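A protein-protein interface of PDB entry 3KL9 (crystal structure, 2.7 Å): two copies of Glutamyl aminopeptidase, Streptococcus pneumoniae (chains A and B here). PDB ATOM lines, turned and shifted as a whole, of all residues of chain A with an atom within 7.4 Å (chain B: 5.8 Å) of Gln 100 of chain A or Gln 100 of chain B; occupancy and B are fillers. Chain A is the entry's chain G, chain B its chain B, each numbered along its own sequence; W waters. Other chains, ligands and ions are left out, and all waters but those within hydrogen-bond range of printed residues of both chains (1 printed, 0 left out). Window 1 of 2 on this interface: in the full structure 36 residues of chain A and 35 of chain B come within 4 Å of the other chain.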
ATOM      1  N   PHE A  73     -18.211  33.351 -24.331  1.00  0.00           N
ATOM      2  CA  PHE A  73     -16.885  33.538 -23.762  1.00  0.00           C
ATOM      3  C   PHE A  73     -16.160  34.679 -24.455  1.00  0.00           C
ATOM      4  O   PHE A  73     -16.676  35.264 -25.416  1.00  0.00           O
ATOM      5  CB  PHE A  73     -16.084  32.235 -23.841  1.00  0.00           C
ATOM      6  CG  PHE A  73     -16.659  31.138 -22.995  1.00  0.00           C
ATOM      7  CD1 PHE A  73     -17.513  30.189 -23.552  1.00  0.00           C
ATOM      8  CD2 PHE A  73     -16.386  31.083 -21.624  1.00  0.00           C
ATOM      9  CE1 PHE A  73     -18.070  29.193 -22.767  1.00  0.00           C
ATOM     10  CE2 PHE A  73     -16.937  30.085 -20.832  1.00  0.00           C
ATOM     11  CZ  PHE A  73     -17.779  29.136 -21.408  1.00  0.00           C
ATOM     12  N   TRP A  92     -21.665  30.303 -16.553  1.00  0.00           N
ATOM     13  CA  TRP A  92     -21.637  28.945 -17.083  1.00  0.00           C
ATOM     14  C   TRP A  92     -21.327  27.946 -15.977  1.00  0.00           C
ATOM     15  O   TRP A  92     -20.421  28.158 -15.167  1.00  0.00           O
ATOM     16  CB  TRP A  92     -20.562  28.792 -18.151  1.00  0.00           C
ATOM     17  CG  TRP A  92     -20.853  29.404 -19.471  1.00  0.00           C
ATOM     18  CD1 TRP A  92     -20.715  30.714 -19.807  1.00  0.00           C
ATOM     19  CD2 TRP A  92     -21.278  28.725 -20.664  1.00  0.00           C
ATOM     20  NE1 TRP A  92     -21.043  30.901 -21.126  1.00  0.00           N
ATOM     21  CE2 TRP A  92     -21.389  29.696 -21.677  1.00  0.00           C
ATOM     22  CE3 TRP A  92     -21.586  27.395 -20.968  1.00  0.00           C
ATOM     23  CZ2 TRP A  92     -21.798  29.379 -22.982  1.00  0.00           C
ATOM     24  CZ3 TRP A  92     -21.987  27.082 -22.264  1.00  0.00           C
ATOM     25  CH2 TRP A  92     -22.091  28.072 -23.252  1.00  0.00           C
ATOM     26  N   MET A  95     -19.266  22.258 -16.002  1.00  0.00           N
ATOM     27  CA  MET A  95     -19.506  20.881 -16.459  1.00  0.00           C
ATOM     28  C   MET A  95     -19.948  20.764 -17.918  1.00  0.00           C
ATOM     29  O   MET A  95     -19.815  19.689 -18.518  1.00  0.00           O
ATOM     30  CB  MET A  95     -20.568  20.194 -15.581  1.00  0.00           C
ATOM     31  CG  MET A  95     -20.227  20.091 -14.102  1.00  0.00           C
ATOM     32  SD  MET A  95     -18.652  19.268 -13.789  1.00  0.00           S
ATOM     33  CE  MET A  95     -19.007  17.654 -14.510  1.00  0.00           C
ATOM     34  N   VAL A  96     -20.492  21.856 -18.462  1.00  0.00           N
ATOM     35  CA  VAL A  96     -21.091  21.871 -19.799  1.00  0.00           C
ATOM     36  C   VAL A  96     -20.181  22.567 -20.812  1.00  0.00           C
ATOM     37  O   VAL A  96     -20.573  22.820 -21.951  1.00  0.00           O
ATOM     38  CB  VAL A  96     -22.526  22.545 -19.807  1.00  0.00           C
ATOM     39  CG1 VAL A  96     -23.475  21.873 -18.817  1.00  0.00           C
ATOM     40  CG2 VAL A  96     -22.457  24.039 -19.525  1.00  0.00           C
ATOM     41  N   VAL A  97     -18.957  22.858 -20.401  1.00  0.00           N
ATOM     42  CA  VAL A  97     -18.101  23.761 -21.157  1.00  0.00           C
ATOM     43  C   VAL A  97     -17.122  23.020 -22.079  1.00  0.00           C
ATOM     44  O   VAL A  97     -16.812  23.479 -23.187  1.00  0.00           O
ATOM     45  CB  VAL A  97     -17.383  24.744 -20.193  1.00  0.00           C
ATOM     46  CG1 VAL A  97     -16.399  25.629 -20.927  1.00  0.00           C
ATOM     47  CG2 VAL A  97     -18.411  25.593 -19.474  1.00  0.00           C
ATOM     48  N   SER A  98     -16.661  21.858 -21.625  1.00  0.00           N
ATOM     49  CA  SER A  98     -15.681  21.070 -22.366  1.00  0.00           C
ATOM     50  C   SER A  98     -16.275  20.457 -23.628  1.00  0.00           C
ATOM     51  O   SER A  98     -17.454  20.108 -23.654  1.00  0.00           O
ATOM     52  CB  SER A  98     -15.102  19.974 -21.472  1.00  0.00           C
ATOM     53  OG  SER A  98     -14.670  20.509 -20.239  1.00  0.00           O
ATOM     54  N   SER A  99     -15.440  20.346 -24.665  1.00  0.00           N
ATOM     55  CA  SER A  99     -15.794  19.707 -25.946  1.00  0.00           C
ATOM     56  C   SER A  99     -17.016  20.318 -26.630  1.00  0.00           C
ATOM     57  O   SER A  99     -17.955  19.604 -27.008  1.00  0.00           O
ATOM     58  CB  SER A  99     -15.966  18.199 -25.763  1.00  0.00           C
ATOM     59  OG  SER A  99     -14.748  17.618 -25.345  1.00  0.00           O
ATOM     60  N   GLN A 100     -16.985  21.640 -26.791  1.00  0.00           N
ATOM     61  CA  GLN A 100     -18.093  22.392 -27.382  1.00  0.00           C
ATOM     62  C   GLN A 100     -17.640  23.218 -28.584  1.00  0.00           C
ATOM     63  O   GLN A 100     -16.556  23.786 -28.557  1.00  0.00           O
ATOM     64  CB  GLN A 100     -18.727  23.304 -26.332  1.00  0.00           C
ATOM     65  CG  GLN A 100     -19.442  22.577 -25.188  1.00  0.00           C
ATOM     66  CD  GLN A 100     -20.794  21.975 -25.580  1.00  0.00           C
ATOM     67  OE1 GLN A 100     -21.259  22.085 -26.729  1.00  0.00           O
ATOM     68  NE2 GLN A 100     -21.431  21.336 -24.617  1.00  0.00           N
ATOM     69  N   ARG A 101     -18.466  23.273 -29.630  1.00  0.00           N
ATOM     70  CA  ARG A 101     -18.198  24.121 -30.797  1.00  0.00           C
ATOM     71  C   ARG A 101     -18.557  25.580 -30.561  1.00  0.00           C
ATOM     72  O   ARG A 101     -19.563  25.884 -29.920  1.00  0.00           O
ATOM     73  CB  ARG A 101     -18.976  23.642 -32.022  1.00  0.00           C
ATOM     74  CG  ARG A 101     -18.151  22.901 -33.056  1.00  0.00           C
ATOM     75  CD  ARG A 101     -18.442  23.452 -34.426  1.00  0.00           C
ATOM     76  NE  ARG A 101     -18.872  22.471 -35.434  1.00  0.00           N
ATOM     77  CZ  ARG A 101     -18.511  21.195 -35.494  1.00  0.00           C
ATOM     78  NH1 ARG A 101     -17.683  20.664 -34.604  1.00  0.00           N
ATOM     79  NH2 ARG A 101     -18.989  20.442 -36.472  1.00  0.00           N
ATOM     80  N   PHE A 102     -17.747  26.477 -31.112  1.00  0.00           N
ATOM     81  CA  PHE A 102     -17.989  27.910 -31.006  1.00  0.00           C
ATOM     82  C   PHE A 102     -17.636  28.644 -32.293  1.00  0.00           C
ATOM     83  O   PHE A 102     -17.036  28.081 -33.221  1.00  0.00           O
ATOM     84  CB  PHE A 102     -17.148  28.524 -29.884  1.00  0.00           C
ATOM     85  CG  PHE A 102     -17.471  28.018 -28.523  1.00  0.00           C
ATOM     86  CD1 PHE A 102     -18.483  28.602 -27.774  1.00  0.00           C
ATOM     87  CD2 PHE A 102     -16.742  26.982 -27.970  1.00  0.00           C
ATOM     88  CE1 PHE A 102     -18.782  28.143 -26.496  1.00  0.00           C
ATOM     89  CE2 PHE A 102     -17.028  26.517 -26.699  1.00  0.00           C
ATOM     90  CZ  PHE A 102     -18.052  27.100 -25.956  1.00  0.00           C
ATOM     91  N   LYS A 103     -18.003  29.919 -32.326  1.00  0.00           N
ATOM     92  CA  LYS A 103     -17.556  30.820 -33.366  1.00  0.00           C
ATOM     93  C   LYS A 103     -16.886  32.009 -32.708  1.00  0.00           C
ATOM     94  O   LYS A 103     -17.475  32.653 -31.836  1.00  0.00           O
ATOM     95  CB  LYS A 103     -18.724  31.260 -34.254  1.00  0.00           C
ATOM     96  CG  LYS A 103     -19.170  30.185 -35.235  1.00  0.00           C
ATOM     97  CD  LYS A 103     -20.366  30.631 -36.061  1.00  0.00           C
ATOM     98  CE  LYS A 103     -20.635  29.639 -37.205  1.00  0.00           C
ATOM     99  NZ  LYS A 103     -21.335  30.301 -38.354  1.00  0.00           N
ATOM    100  N   VAL A 114     -13.872  27.606 -33.364  1.00  0.00           N
ATOM    101  CA  VAL A 114     -13.109  27.411 -32.137  1.00  0.00           C
ATOM    102  C   VAL A 114     -13.817  26.381 -31.280  1.00  0.00           C
ATOM    103  O   VAL A 114     -15.035  26.406 -31.150  1.00  0.00           O
ATOM    104  CB  VAL A 114     -12.943  28.747 -31.366  1.00  0.00           C
ATOM    105  CG1 VAL A 114     -12.445  28.522 -29.945  1.00  0.00           C
ATOM    106  CG2 VAL A 114     -11.998  29.654 -32.103  1.00  0.00           C
ATOM    107  N   ILE A 115     -13.054  25.458 -30.714  1.00  0.00           N
ATOM    108  CA  ILE A 115     -13.617  24.457 -29.821  1.00  0.00           C
ATOM    109  C   ILE A 115     -12.905  24.452 -28.474  1.00  0.00           C
ATOM    110  O   ILE A 115     -11.709  24.752 -28.392  1.00  0.00           O
ATOM    111  CB  ILE A 115     -13.595  23.019 -30.439  1.00  0.00           C
ATOM    112  CG1 ILE A 115     -12.166  22.611 -30.855  1.00  0.00           C
ATOM    113  CG2 ILE A 115     -14.599  22.911 -31.594  1.00  0.00           C
ATOM    114  CD1 ILE A 115     -11.904  21.112 -30.822  1.00  0.00           C
ATOM    115  N   SER A 116     -13.643  24.122 -27.418  1.00  0.00           N
ATOM    116  CA  SER A 116     -13.024  23.896 -26.125  1.00  0.00           C
ATOM    117  C   SER A 116     -12.566  22.442 -26.055  1.00  0.00           C
ATOM    118  O   SER A 116     -13.228  21.560 -26.586  1.00  0.00           O
ATOM    119  CB  SER A 116     -13.983  24.247 -24.992  1.00  0.00           C
ATOM    120  OG  SER A 116     -15.195  23.525 -25.111  1.00  0.00           O
ATOM    121  N   GLY A 117     -11.421  22.203 -25.418  1.00  0.00           N
ATOM    122  CA  GLY A 117     -10.843  20.864 -25.312  1.00  0.00           C
ATOM    123  C   GLY A 117     -11.594  19.926 -24.386  1.00  0.00           C
ATOM    124  O   GLY A 117     -12.160  20.350 -23.375  1.00  0.00           O
ATOM    125  N   PHE A 140      -9.036  26.490 -25.248  1.00  0.00           N
ATOM    126  CA  PHE A 140      -9.828  26.849 -26.427  1.00  0.00           C
ATOM    127  C   PHE A 140      -8.936  26.828 -27.664  1.00  0.00           C
ATOM    128  O   PHE A 140      -7.846  27.389 -27.664  1.00  0.00           O
ATOM    129  CB  PHE A 140     -10.524  28.202 -26.238  1.00  0.00           C
ATOM    130  CG  PHE A 140     -11.782  28.122 -25.409  1.00  0.00           C
ATOM    131  CD1 PHE A 140     -11.717  27.891 -24.037  1.00  0.00           C
ATOM    132  CD2 PHE A 140     -13.029  28.267 -26.004  1.00  0.00           C
ATOM    133  CE1 PHE A 140     -12.868  27.806 -23.267  1.00  0.00           C
ATOM    134  CE2 PHE A 140     -14.190  28.188 -25.249  1.00  0.00           C
ATOM    135  CZ  PHE A 140     -14.107  27.959 -23.867  1.00  0.00           C
ATOM    136  N   ASP A 141      -9.413  26.169 -28.712  1.00  0.00           N
ATOM    137  CA  ASP A 141      -8.565  25.748 -29.814  1.00  0.00           C
ATOM    138  C   ASP A 141      -9.178  26.131 -31.158  1.00  0.00           C
ATOM    139  O   ASP A 141     -10.329  25.796 -31.433  1.00  0.00           O
ATOM    140  CB  ASP A 141      -8.383  24.226 -29.735  1.00  0.00           C
ATOM    141  CG  ASP A 141      -7.171  23.717 -30.508  1.00  0.00           C
ATOM    142  OD1 ASP A 141      -6.735  22.586 -30.208  1.00  0.00           O
ATOM    143  OD2 ASP A 141      -6.660  24.419 -31.410  1.00  0.00           O
ATOM    144  N   PRO A 163     -21.343  30.317 -28.721  1.00  0.00           N
ATOM    145  CA  PRO A 163     -21.774  28.931 -28.931  1.00  0.00           C
ATOM    146  C   PRO A 163     -22.229  28.671 -30.367  1.00  0.00           C
ATOM    147  O   PRO A 163     -22.841  29.535 -30.986  1.00  0.00           O
ATOM    148  CB  PRO A 163     -22.952  28.794 -27.972  1.00  0.00           C
ATOM    149  CG  PRO A 163     -22.574  29.667 -26.845  1.00  0.00           C
ATOM    150  CD  PRO A 163     -21.860  30.851 -27.447  1.00  0.00           C
ATOM    151  N   ASP A 164     -21.909  27.492 -30.889  1.00  0.00           N
ATOM    152  CA  ASP A 164     -22.262  27.123 -32.263  1.00  0.00           C
ATOM    153  C   ASP A 164     -23.212  25.933 -32.214  1.00  0.00           C
ATOM    154  O   ASP A 164     -22.801  24.805 -31.954  1.00  0.00           O
ATOM    155  CB  ASP A 164     -20.988  26.814 -33.067  1.00  0.00           C
ATOM    156  CG  ASP A 164     -21.268  26.368 -34.495  1.00  0.00           C
ATOM    157  OD1 ASP A 164     -22.392  26.589 -34.993  1.00  0.00           O
ATOM    158  OD2 ASP A 164     -20.348  25.795 -35.125  1.00  0.00           O
ATOM    159  N   SER A 165     -24.490  26.198 -32.453  1.00  0.00           N
ATOM    160  CA  SER A 165     -25.532  25.205 -32.240  1.00  0.00           C
ATOM    161  C   SER A 165     -26.773  25.544 -33.062  1.00  0.00           C
ATOM    162  O   SER A 165     -27.280  26.667 -33.017  1.00  0.00           O
ATOM    163  CB  SER A 165     -25.882  25.143 -30.748  1.00  0.00           C
ATOM    164  OG  SER A 165     -26.805  24.109 -30.457  1.00  0.00           O
ATOM    165  N   ILE A 177     -34.840  21.990 -29.600  1.00  0.00           N
ATOM    166  CA  ILE A 177     -33.488  21.954 -29.069  1.00  0.00           C
ATOM    167  C   ILE A 177     -32.696  23.024 -29.807  1.00  0.00           C
ATOM    168  O   ILE A 177     -32.626  23.004 -31.042  1.00  0.00           O
ATOM    169  CB  ILE A 177     -32.826  20.570 -29.279  1.00  0.00           C
ATOM    170  CG1 ILE A 177     -33.531  19.495 -28.443  1.00  0.00           C
ATOM    171  CG2 ILE A 177     -31.367  20.628 -28.922  1.00  0.00           C
ATOM    172  CD1 ILE A 177     -33.394  18.075 -28.985  1.00  0.00           C
ATOM    173  N   SER A 320     -26.584  26.972 -22.020  1.00  0.00           N
ATOM    174  CA  SER A 320     -25.788  25.902 -22.630  1.00  0.00           C
ATOM    175  C   SER A 320     -26.005  25.859 -24.141  1.00  0.00           C
ATOM    176  O   SER A 320     -26.659  26.740 -24.695  1.00  0.00           O
ATOM    177  CB  SER A 320     -26.049  24.535 -21.968  1.00  0.00           C
ATOM    178  OG  SER A 320     -27.158  23.847 -22.523  1.00  0.00           O
ATOM    179  N   HIS A 321     -25.422  24.865 -24.806  1.00  0.00           N
ATOM    180  CA  HIS A 321     -25.572  24.716 -26.254  1.00  0.00           C
ATOM    181  C   HIS A 321     -26.882  24.024 -26.580  1.00  0.00           C
ATOM    182  O   HIS A 321     -27.421  24.175 -27.679  1.00  0.00           O
ATOM    183  CB  HIS A 321     -24.424  23.890 -26.821  1.00  0.00           C
ATOM    184  CG  HIS A 321     -23.117  24.614 -26.853  1.00  0.00           C
ATOM    185  ND1 HIS A 321     -22.489  24.957 -28.030  1.00  0.00           N
ATOM    186  CD2 HIS A 321     -22.319  25.058 -25.855  1.00  0.00           C
ATOM    187  CE1 HIS A 321     -21.357  25.579 -27.755  1.00  0.00           C
ATOM    188  NE2 HIS A 321     -21.232  25.654 -26.442  1.00  0.00           N
ATOM    189  N   GLN A 322     -27.379  23.267 -25.604  1.00  0.00           N
ATOM    190  CA  GLN A 322     -28.539  22.406 -25.767  1.00  0.00           C
ATOM    191  C   GLN A 322     -29.673  22.750 -24.794  1.00  0.00           C
ATOM    192  O   GLN A 322     -29.799  22.162 -23.715  1.00  0.00           O
ATOM    193  CB  GLN A 322     -28.120  20.941 -25.613  1.00  0.00           C
ATOM    194  CG  GLN A 322     -26.927  20.523 -26.474  1.00  0.00           C
ATOM    195  CD  GLN A 322     -27.149  20.783 -27.952  1.00  0.00           C
ATOM    196  OE1 GLN A 322     -26.201  20.936 -28.724  1.00  0.00           O
ATOM    197  NE2 GLN A 322     -28.406  20.844 -28.352  1.00  0.00           N
ATOM    198  N   VAL B  96     -17.074  15.933 -20.330  1.00  0.00           N
ATOM    199  CA  VAL B  96     -17.411  16.320 -21.701  1.00  0.00           C
ATOM    200  C   VAL B  96     -18.838  15.924 -22.078  1.00  0.00           C
ATOM    201  O   VAL B  96     -19.336  16.331 -23.124  1.00  0.00           O
ATOM    202  CB  VAL B  96     -16.383  15.777 -22.764  1.00  0.00           C
ATOM    203  CG1 VAL B  96     -14.952  16.065 -22.344  1.00  0.00           C
ATOM    204  CG2 VAL B  96     -16.557  14.288 -23.011  1.00  0.00           C
ATOM    205  N   VAL B  97     -19.495  15.162 -21.208  1.00  0.00           N
ATOM    206  CA  VAL B  97     -20.763  14.513 -21.537  1.00  0.00           C
ATOM    207  C   VAL B  97     -21.993  15.423 -21.438  1.00  0.00           C
ATOM    208  O   VAL B  97     -22.968  15.239 -22.169  1.00  0.00           O
ATOM    209  CB  VAL B  97     -20.961  13.231 -20.686  1.00  0.00           C
ATOM    210  CG1 VAL B  97     -22.275  12.533 -21.027  1.00  0.00           C
ATOM    211  CG2 VAL B  97     -19.789  12.277 -20.896  1.00  0.00           C
ATOM    212  N   SER B  98     -21.949  16.410 -20.549  1.00  0.00           N
ATOM    213  CA  SER B  98     -23.118  17.257 -20.318  1.00  0.00           C
ATOM    214  C   SER B  98     -23.372  18.204 -21.478  1.00  0.00           C
ATOM    215  O   SER B  98     -22.434  18.634 -22.142  1.00  0.00           O
ATOM    216  CB  SER B  98     -22.958  18.040 -19.019  1.00  0.00           C
ATOM    217  OG  SER B  98     -22.846  17.152 -17.925  1.00  0.00           O
ATOM    218  N   SER B  99     -24.646  18.516 -21.710  1.00  0.00           N
ATOM    219  CA  SER B  99     -25.074  19.449 -22.762  1.00  0.00           C
ATOM    220  C   SER B  99     -24.504  19.134 -24.152  1.00  0.00           C
ATOM    221  O   SER B  99     -23.797  19.942 -24.746  1.00  0.00           O
ATOM    222  CB  SER B  99     -24.794  20.897 -22.355  1.00  0.00           C
ATOM    223  OG  SER B  99     -25.674  21.304 -21.323  1.00  0.00           O
ATOM    224  N   GLN B 100     -24.841  17.953 -24.662  1.00  0.00           N
ATOM    225  CA  GLN B 100     -24.339  17.480 -25.937  1.00  0.00           C
ATOM    226  C   GLN B 100     -25.469  16.916 -26.796  1.00  0.00           C
ATOM    227  O   GLN B 100     -26.424  16.346 -26.274  1.00  0.00           O
ATOM    228  CB  GLN B 100     -23.272  16.405 -25.705  1.00  0.00           C
ATOM    229  CG  GLN B 100     -22.015  16.886 -24.985  1.00  0.00           C
ATOM    230  CD  GLN B 100     -21.039  17.620 -25.893  1.00  0.00           C
ATOM    231  OE1 GLN B 100     -21.298  17.830 -27.080  1.00  0.00           O
ATOM    232  NE2 GLN B 100     -19.908  18.011 -25.336  1.00  0.00           N
ATOM    233  N   ARG B 101     -25.350  17.080 -28.112  1.00  0.00           N
ATOM    234  CA  ARG B 101     -26.321  16.527 -29.053  1.00  0.00           C
ATOM    235  C   ARG B 101     -25.969  15.124 -29.487  1.00  0.00           C
ATOM    236  O   ARG B 101     -24.795  14.789 -29.692  1.00  0.00           O
ATOM    237  CB  ARG B 101     -26.477  17.399 -30.298  1.00  0.00           C
ATOM    238  CG  ARG B 101     -27.689  18.283 -30.261  1.00  0.00           C
ATOM    239  CD  ARG B 101     -28.500  18.202 -31.525  1.00  0.00           C
ATOM    240  NE  ARG B 101     -28.336  19.362 -32.405  1.00  0.00           N
ATOM    241  CZ  ARG B 101     -28.525  20.633 -32.050  1.00  0.00           C
ATOM    242  NH1 ARG B 101     -28.846  20.963 -30.810  1.00  0.00           N
ATOM    243  NH2 ARG B 101     -28.369  21.588 -32.946  1.00  0.00           N
ATOM    244  N   PHE B 102     -27.017  14.322 -29.648  1.00  0.00           N
ATOM    245  CA  PHE B 102     -26.907  12.927 -30.022  1.00  0.00           C
ATOM    246  C   PHE B 102     -28.038  12.560 -30.980  1.00  0.00           C
ATOM    247  O   PHE B 102     -29.016  13.297 -31.123  1.00  0.00           O
ATOM    248  CB  PHE B 102     -27.022  12.050 -28.777  1.00  0.00           C
ATOM    249  CG  PHE B 102     -25.936  12.257 -27.769  1.00  0.00           C
ATOM    250  CD1 PHE B 102     -24.739  11.555 -27.862  1.00  0.00           C
ATOM    251  CD2 PHE B 102     -26.119  13.123 -26.701  1.00  0.00           C
ATOM    252  CE1 PHE B 102     -23.731  11.735 -26.921  1.00  0.00           C
ATOM    253  CE2 PHE B 102     -25.116  13.307 -25.756  1.00  0.00           C
ATOM    254  CZ  PHE B 102     -23.921  12.611 -25.867  1.00  0.00           C
ATOM    255  N   VAL B 114     -31.723  13.409 -29.412  1.00  0.00           N
ATOM    256  CA  VAL B 114     -31.584  13.348 -27.958  1.00  0.00           C
ATOM    257  C   VAL B 114     -30.424  14.229 -27.520  1.00  0.00           C
ATOM    258  O   VAL B 114     -29.381  14.246 -28.170  1.00  0.00           O
ATOM    259  CB  VAL B 114     -31.346  11.886 -27.462  1.00  0.00           C
ATOM    260  CG1 VAL B 114     -30.657  11.848 -26.098  1.00  0.00           C
ATOM    261  CG2 VAL B 114     -32.649  11.118 -27.407  1.00  0.00           C
ATOM    262  N   ILE B 115     -30.615  14.963 -26.425  1.00  0.00           N
ATOM    263  CA  ILE B 115     -29.529  15.719 -25.793  1.00  0.00           C
ATOM    264  C   ILE B 115     -29.299  15.288 -24.350  1.00  0.00           C
ATOM    265  O   ILE B 115     -30.208  14.780 -23.691  1.00  0.00           O
ATOM    266  CB  ILE B 115     -29.778  17.242 -25.818  1.00  0.00           C
ATOM    267  CG1 ILE B 115     -31.142  17.582 -25.180  1.00  0.00           C
ATOM    268  CG2 ILE B 115     -29.654  17.761 -27.240  1.00  0.00           C
ATOM    269  CD1 ILE B 115     -31.258  19.001 -24.652  1.00  0.00           C
ATOM    270  N   SER B 116     -28.078  15.489 -23.866  1.00  0.00           N
ATOM    271  CA  SER B 116     -27.781  15.289 -22.454  1.00  0.00           C
ATOM    272  C   SER B 116     -27.975  16.604 -21.713  1.00  0.00           C
ATOM    273  O   SER B 116     -27.724  17.674 -22.270  1.00  0.00           O
ATOM    274  CB  SER B 116     -26.356  14.768 -22.265  1.00  0.00           C
ATOM    275  OG  SER B 116     -25.412  15.608 -22.904  1.00  0.00           O
ATOM    276  N   GLY B 117     -28.440  16.529 -20.468  1.00  0.00           N
ATOM    277  CA  GLY B 117     -28.623  17.723 -19.650  1.00  0.00           C
ATOM    278  C   GLY B 117     -27.318  18.182 -19.027  1.00  0.00           C
ATOM    279  O   GLY B 117     -27.296  18.624 -17.878  1.00  0.00           O
ATOM    280  N   HIS B 321     -17.167  15.049 -28.980  1.00  0.00           N
ATOM    281  CA  HIS B 321     -17.842  15.548 -30.170  1.00  0.00           C
ATOM    282  C   HIS B 321     -16.932  16.465 -30.952  1.00  0.00           C
ATOM    283  O   HIS B 321     -17.225  16.784 -32.105  1.00  0.00           O
ATOM    284  CB  HIS B 321     -19.095  16.339 -29.786  1.00  0.00           C
ATOM    285  CG  HIS B 321     -20.123  15.535 -29.059  1.00  0.00           C
ATOM    286  ND1 HIS B 321     -21.389  15.322 -29.562  1.00  0.00           N
ATOM    287  CD2 HIS B 321     -20.081  14.905 -27.862  1.00  0.00           C
ATOM    288  CE1 HIS B 321     -22.081  14.588 -28.709  1.00  0.00           C
ATOM    289  NE2 HIS B 321     -21.309  14.317 -27.672  1.00  0.00           N
ATOM    290  N   GLN B 322     -15.848  16.913 -30.318  1.00  0.00           N
ATOM    291  CA  GLN B 322     -14.953  17.899 -30.925  1.00  0.00           C
ATOM    292  C   GLN B 322     -13.490  17.453 -30.928  1.00  0.00           C
ATOM    293  O   GLN B 322     -12.686  17.881 -30.090  1.00  0.00           O
ATOM    294  CB  GLN B 322     -15.099  19.267 -30.249  1.00  0.00           C
ATOM    295  CG  GLN B 322     -16.531  19.692 -29.961  1.00  0.00           C
ATOM    296  CD  GLN B 322     -17.368  19.921 -31.205  1.00  0.00           C
ATOM    297  OE1 GLN B 322     -18.567  19.664 -31.215  1.00  0.00           O
ATOM    298  NE2 GLN B 322     -16.740  20.408 -32.255  1.00  0.00           N
HETATM  299  O   HOH W   1     -28.161  20.463 -22.084  1.00  0.00           O
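O of Ser 99 of chain B lies within hydrogen-bond range of NE2 of Gln 100 of chain A, 2.7 Å away. OG of Ser 320 of chain A is in hydrogen-bond range of OG of Ser 99 of chain B, at 3.2 Å. NE2 of Gln 100 of chain B lies within hydrogen-bond range of O of Ser 99 of chain A, at 3.0 Å. NH1 of Arg 101 of chain B lies close to NE2 of Gln 322 of chain A (2.5 Å). NH1 of Arg 101 of chain A sits close to NE2 of Gln 322 of chain B.
The backbone NH of Gln 100 of chain B lies within hydrogen-bond range of the side-chain hydroxyl of Ser 116 of chain B, at 3.0 Å. O of Arg 101 of chain B sits close to ND1 of His 321 of chain B, 3.4 Å away. N of Ser 99 of chain A is in hydrogen-bond range of O of Ser 116 of chain A (3.2 Å). The side-chain hydroxyl (OG) of Ser 116 of chain A lies within hydrogen-bond range of the backbone NH (N) of Gln 100 of chain A, 3.1 Å away. OE1 of Gln 100 of chain A lies close to ND1 of His 321 of chain A. The guanidinium group (NE) of Arg 101 of chain A is in salt-bridge range of the side-chain carboxylate (OD2) of Asp 164 of chain A, 3.7 Å away.
CB of Ser 98 of chain B touches O of Met 95 of chain A, at 3.6 Å. Ser 98 of chain B touches Val 96 of chain A (CB to CG1, 3.9 Å). Ser 98 of chain A touches Gln 100 of chain B (O to NE2, 3.6 Å). Gln 322 of chain B touches Ser 99 of chain A (CG to O, 3.3 Å). NE2 of Gln 100 of chain A touches O of Ser 98 of chain B, at 3.8 Å. Gln 100 of chain B touches Gln 100 of chain A (NE2 to NE2, 3.7 Å). CG of Gln 322 of chain B touches N of Gln 100 of chain A, 3.7 Å away. Gln 322 of chain B touches Ile 115 of chain A. Ile 115 of chain B touches Ile 177 of chain A (CG2 to CG2, 3.7 Å). NE2 of Gln 322 of chain A touches CG2 of Ile 115 of chain B, 3.5 Å away.
Of chain B, only Ser 98 (3.8 Å), Ser 99 (2.7 Å), Gln 100 (3.7 Å) and Gln 322 (3.7 Å) come within 4 Å of Gln 100 of chain A. Gln 100 of chain B touches four residues of chain A. Of the printed residues of chain A, Gln 322 of chain B touches Ser 99 (3.3 Å), Gln 100 (3.7 Å), Arg 101 (2.5 Å) and Ile 115 (3.4 Å). Of the printed residues of chain B, Ser 98 of chain A touches Gln 100 (3.6 Å). The nearest residue of chain B that does not touch Gln 100 of chain A is Val 96 of chain B (5.6 Å). The nearest residue of chain A that does not touch Gln 100 of chain B is Val 96 of chain A (5.9 Å).
Hydrophobic or aromatic side chains of chain A that line the printed part of chain B: Val 96, Ile 115 and Ile 177. Hydrophobic or aromatic side chains of chain B within 4 Å of the printed part of chain A: Val 96 and Ile 115. Among the printed residues, 21 pairs touch across the chains.
Val 96 of chain A touches Ser 98 of chain B, but with the chains exchanged Ser 98 of chain A does not touch Val 96 of chain B (4.01 Å). Val 96 of chain A touches Ser 99 of chain B, and with the chains exchanged Ser 99 of chain A touches Val 96 of chain B. Ser 99 of chain A touches Gln 100 of chain B, and with the chains exchanged Gln 100 of chain A touches Ser 99 of chain B. Gln 100 of chain A touches Gln 322 of chain B, and with the chains exchanged Gln 322 of chain A touches Gln 100 of chain B.
Water W1 lies within hydrogen-bond range of the side-chain hydroxyl (OG) of Ser 99 of chain B (2.7 Å), the backbone carbonyl oxygen (O) of Ser 116 of chain B (2.8 Å) and the backbone carbonyl oxygen (O) of Gln 322 of chain A (2.9 Å).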
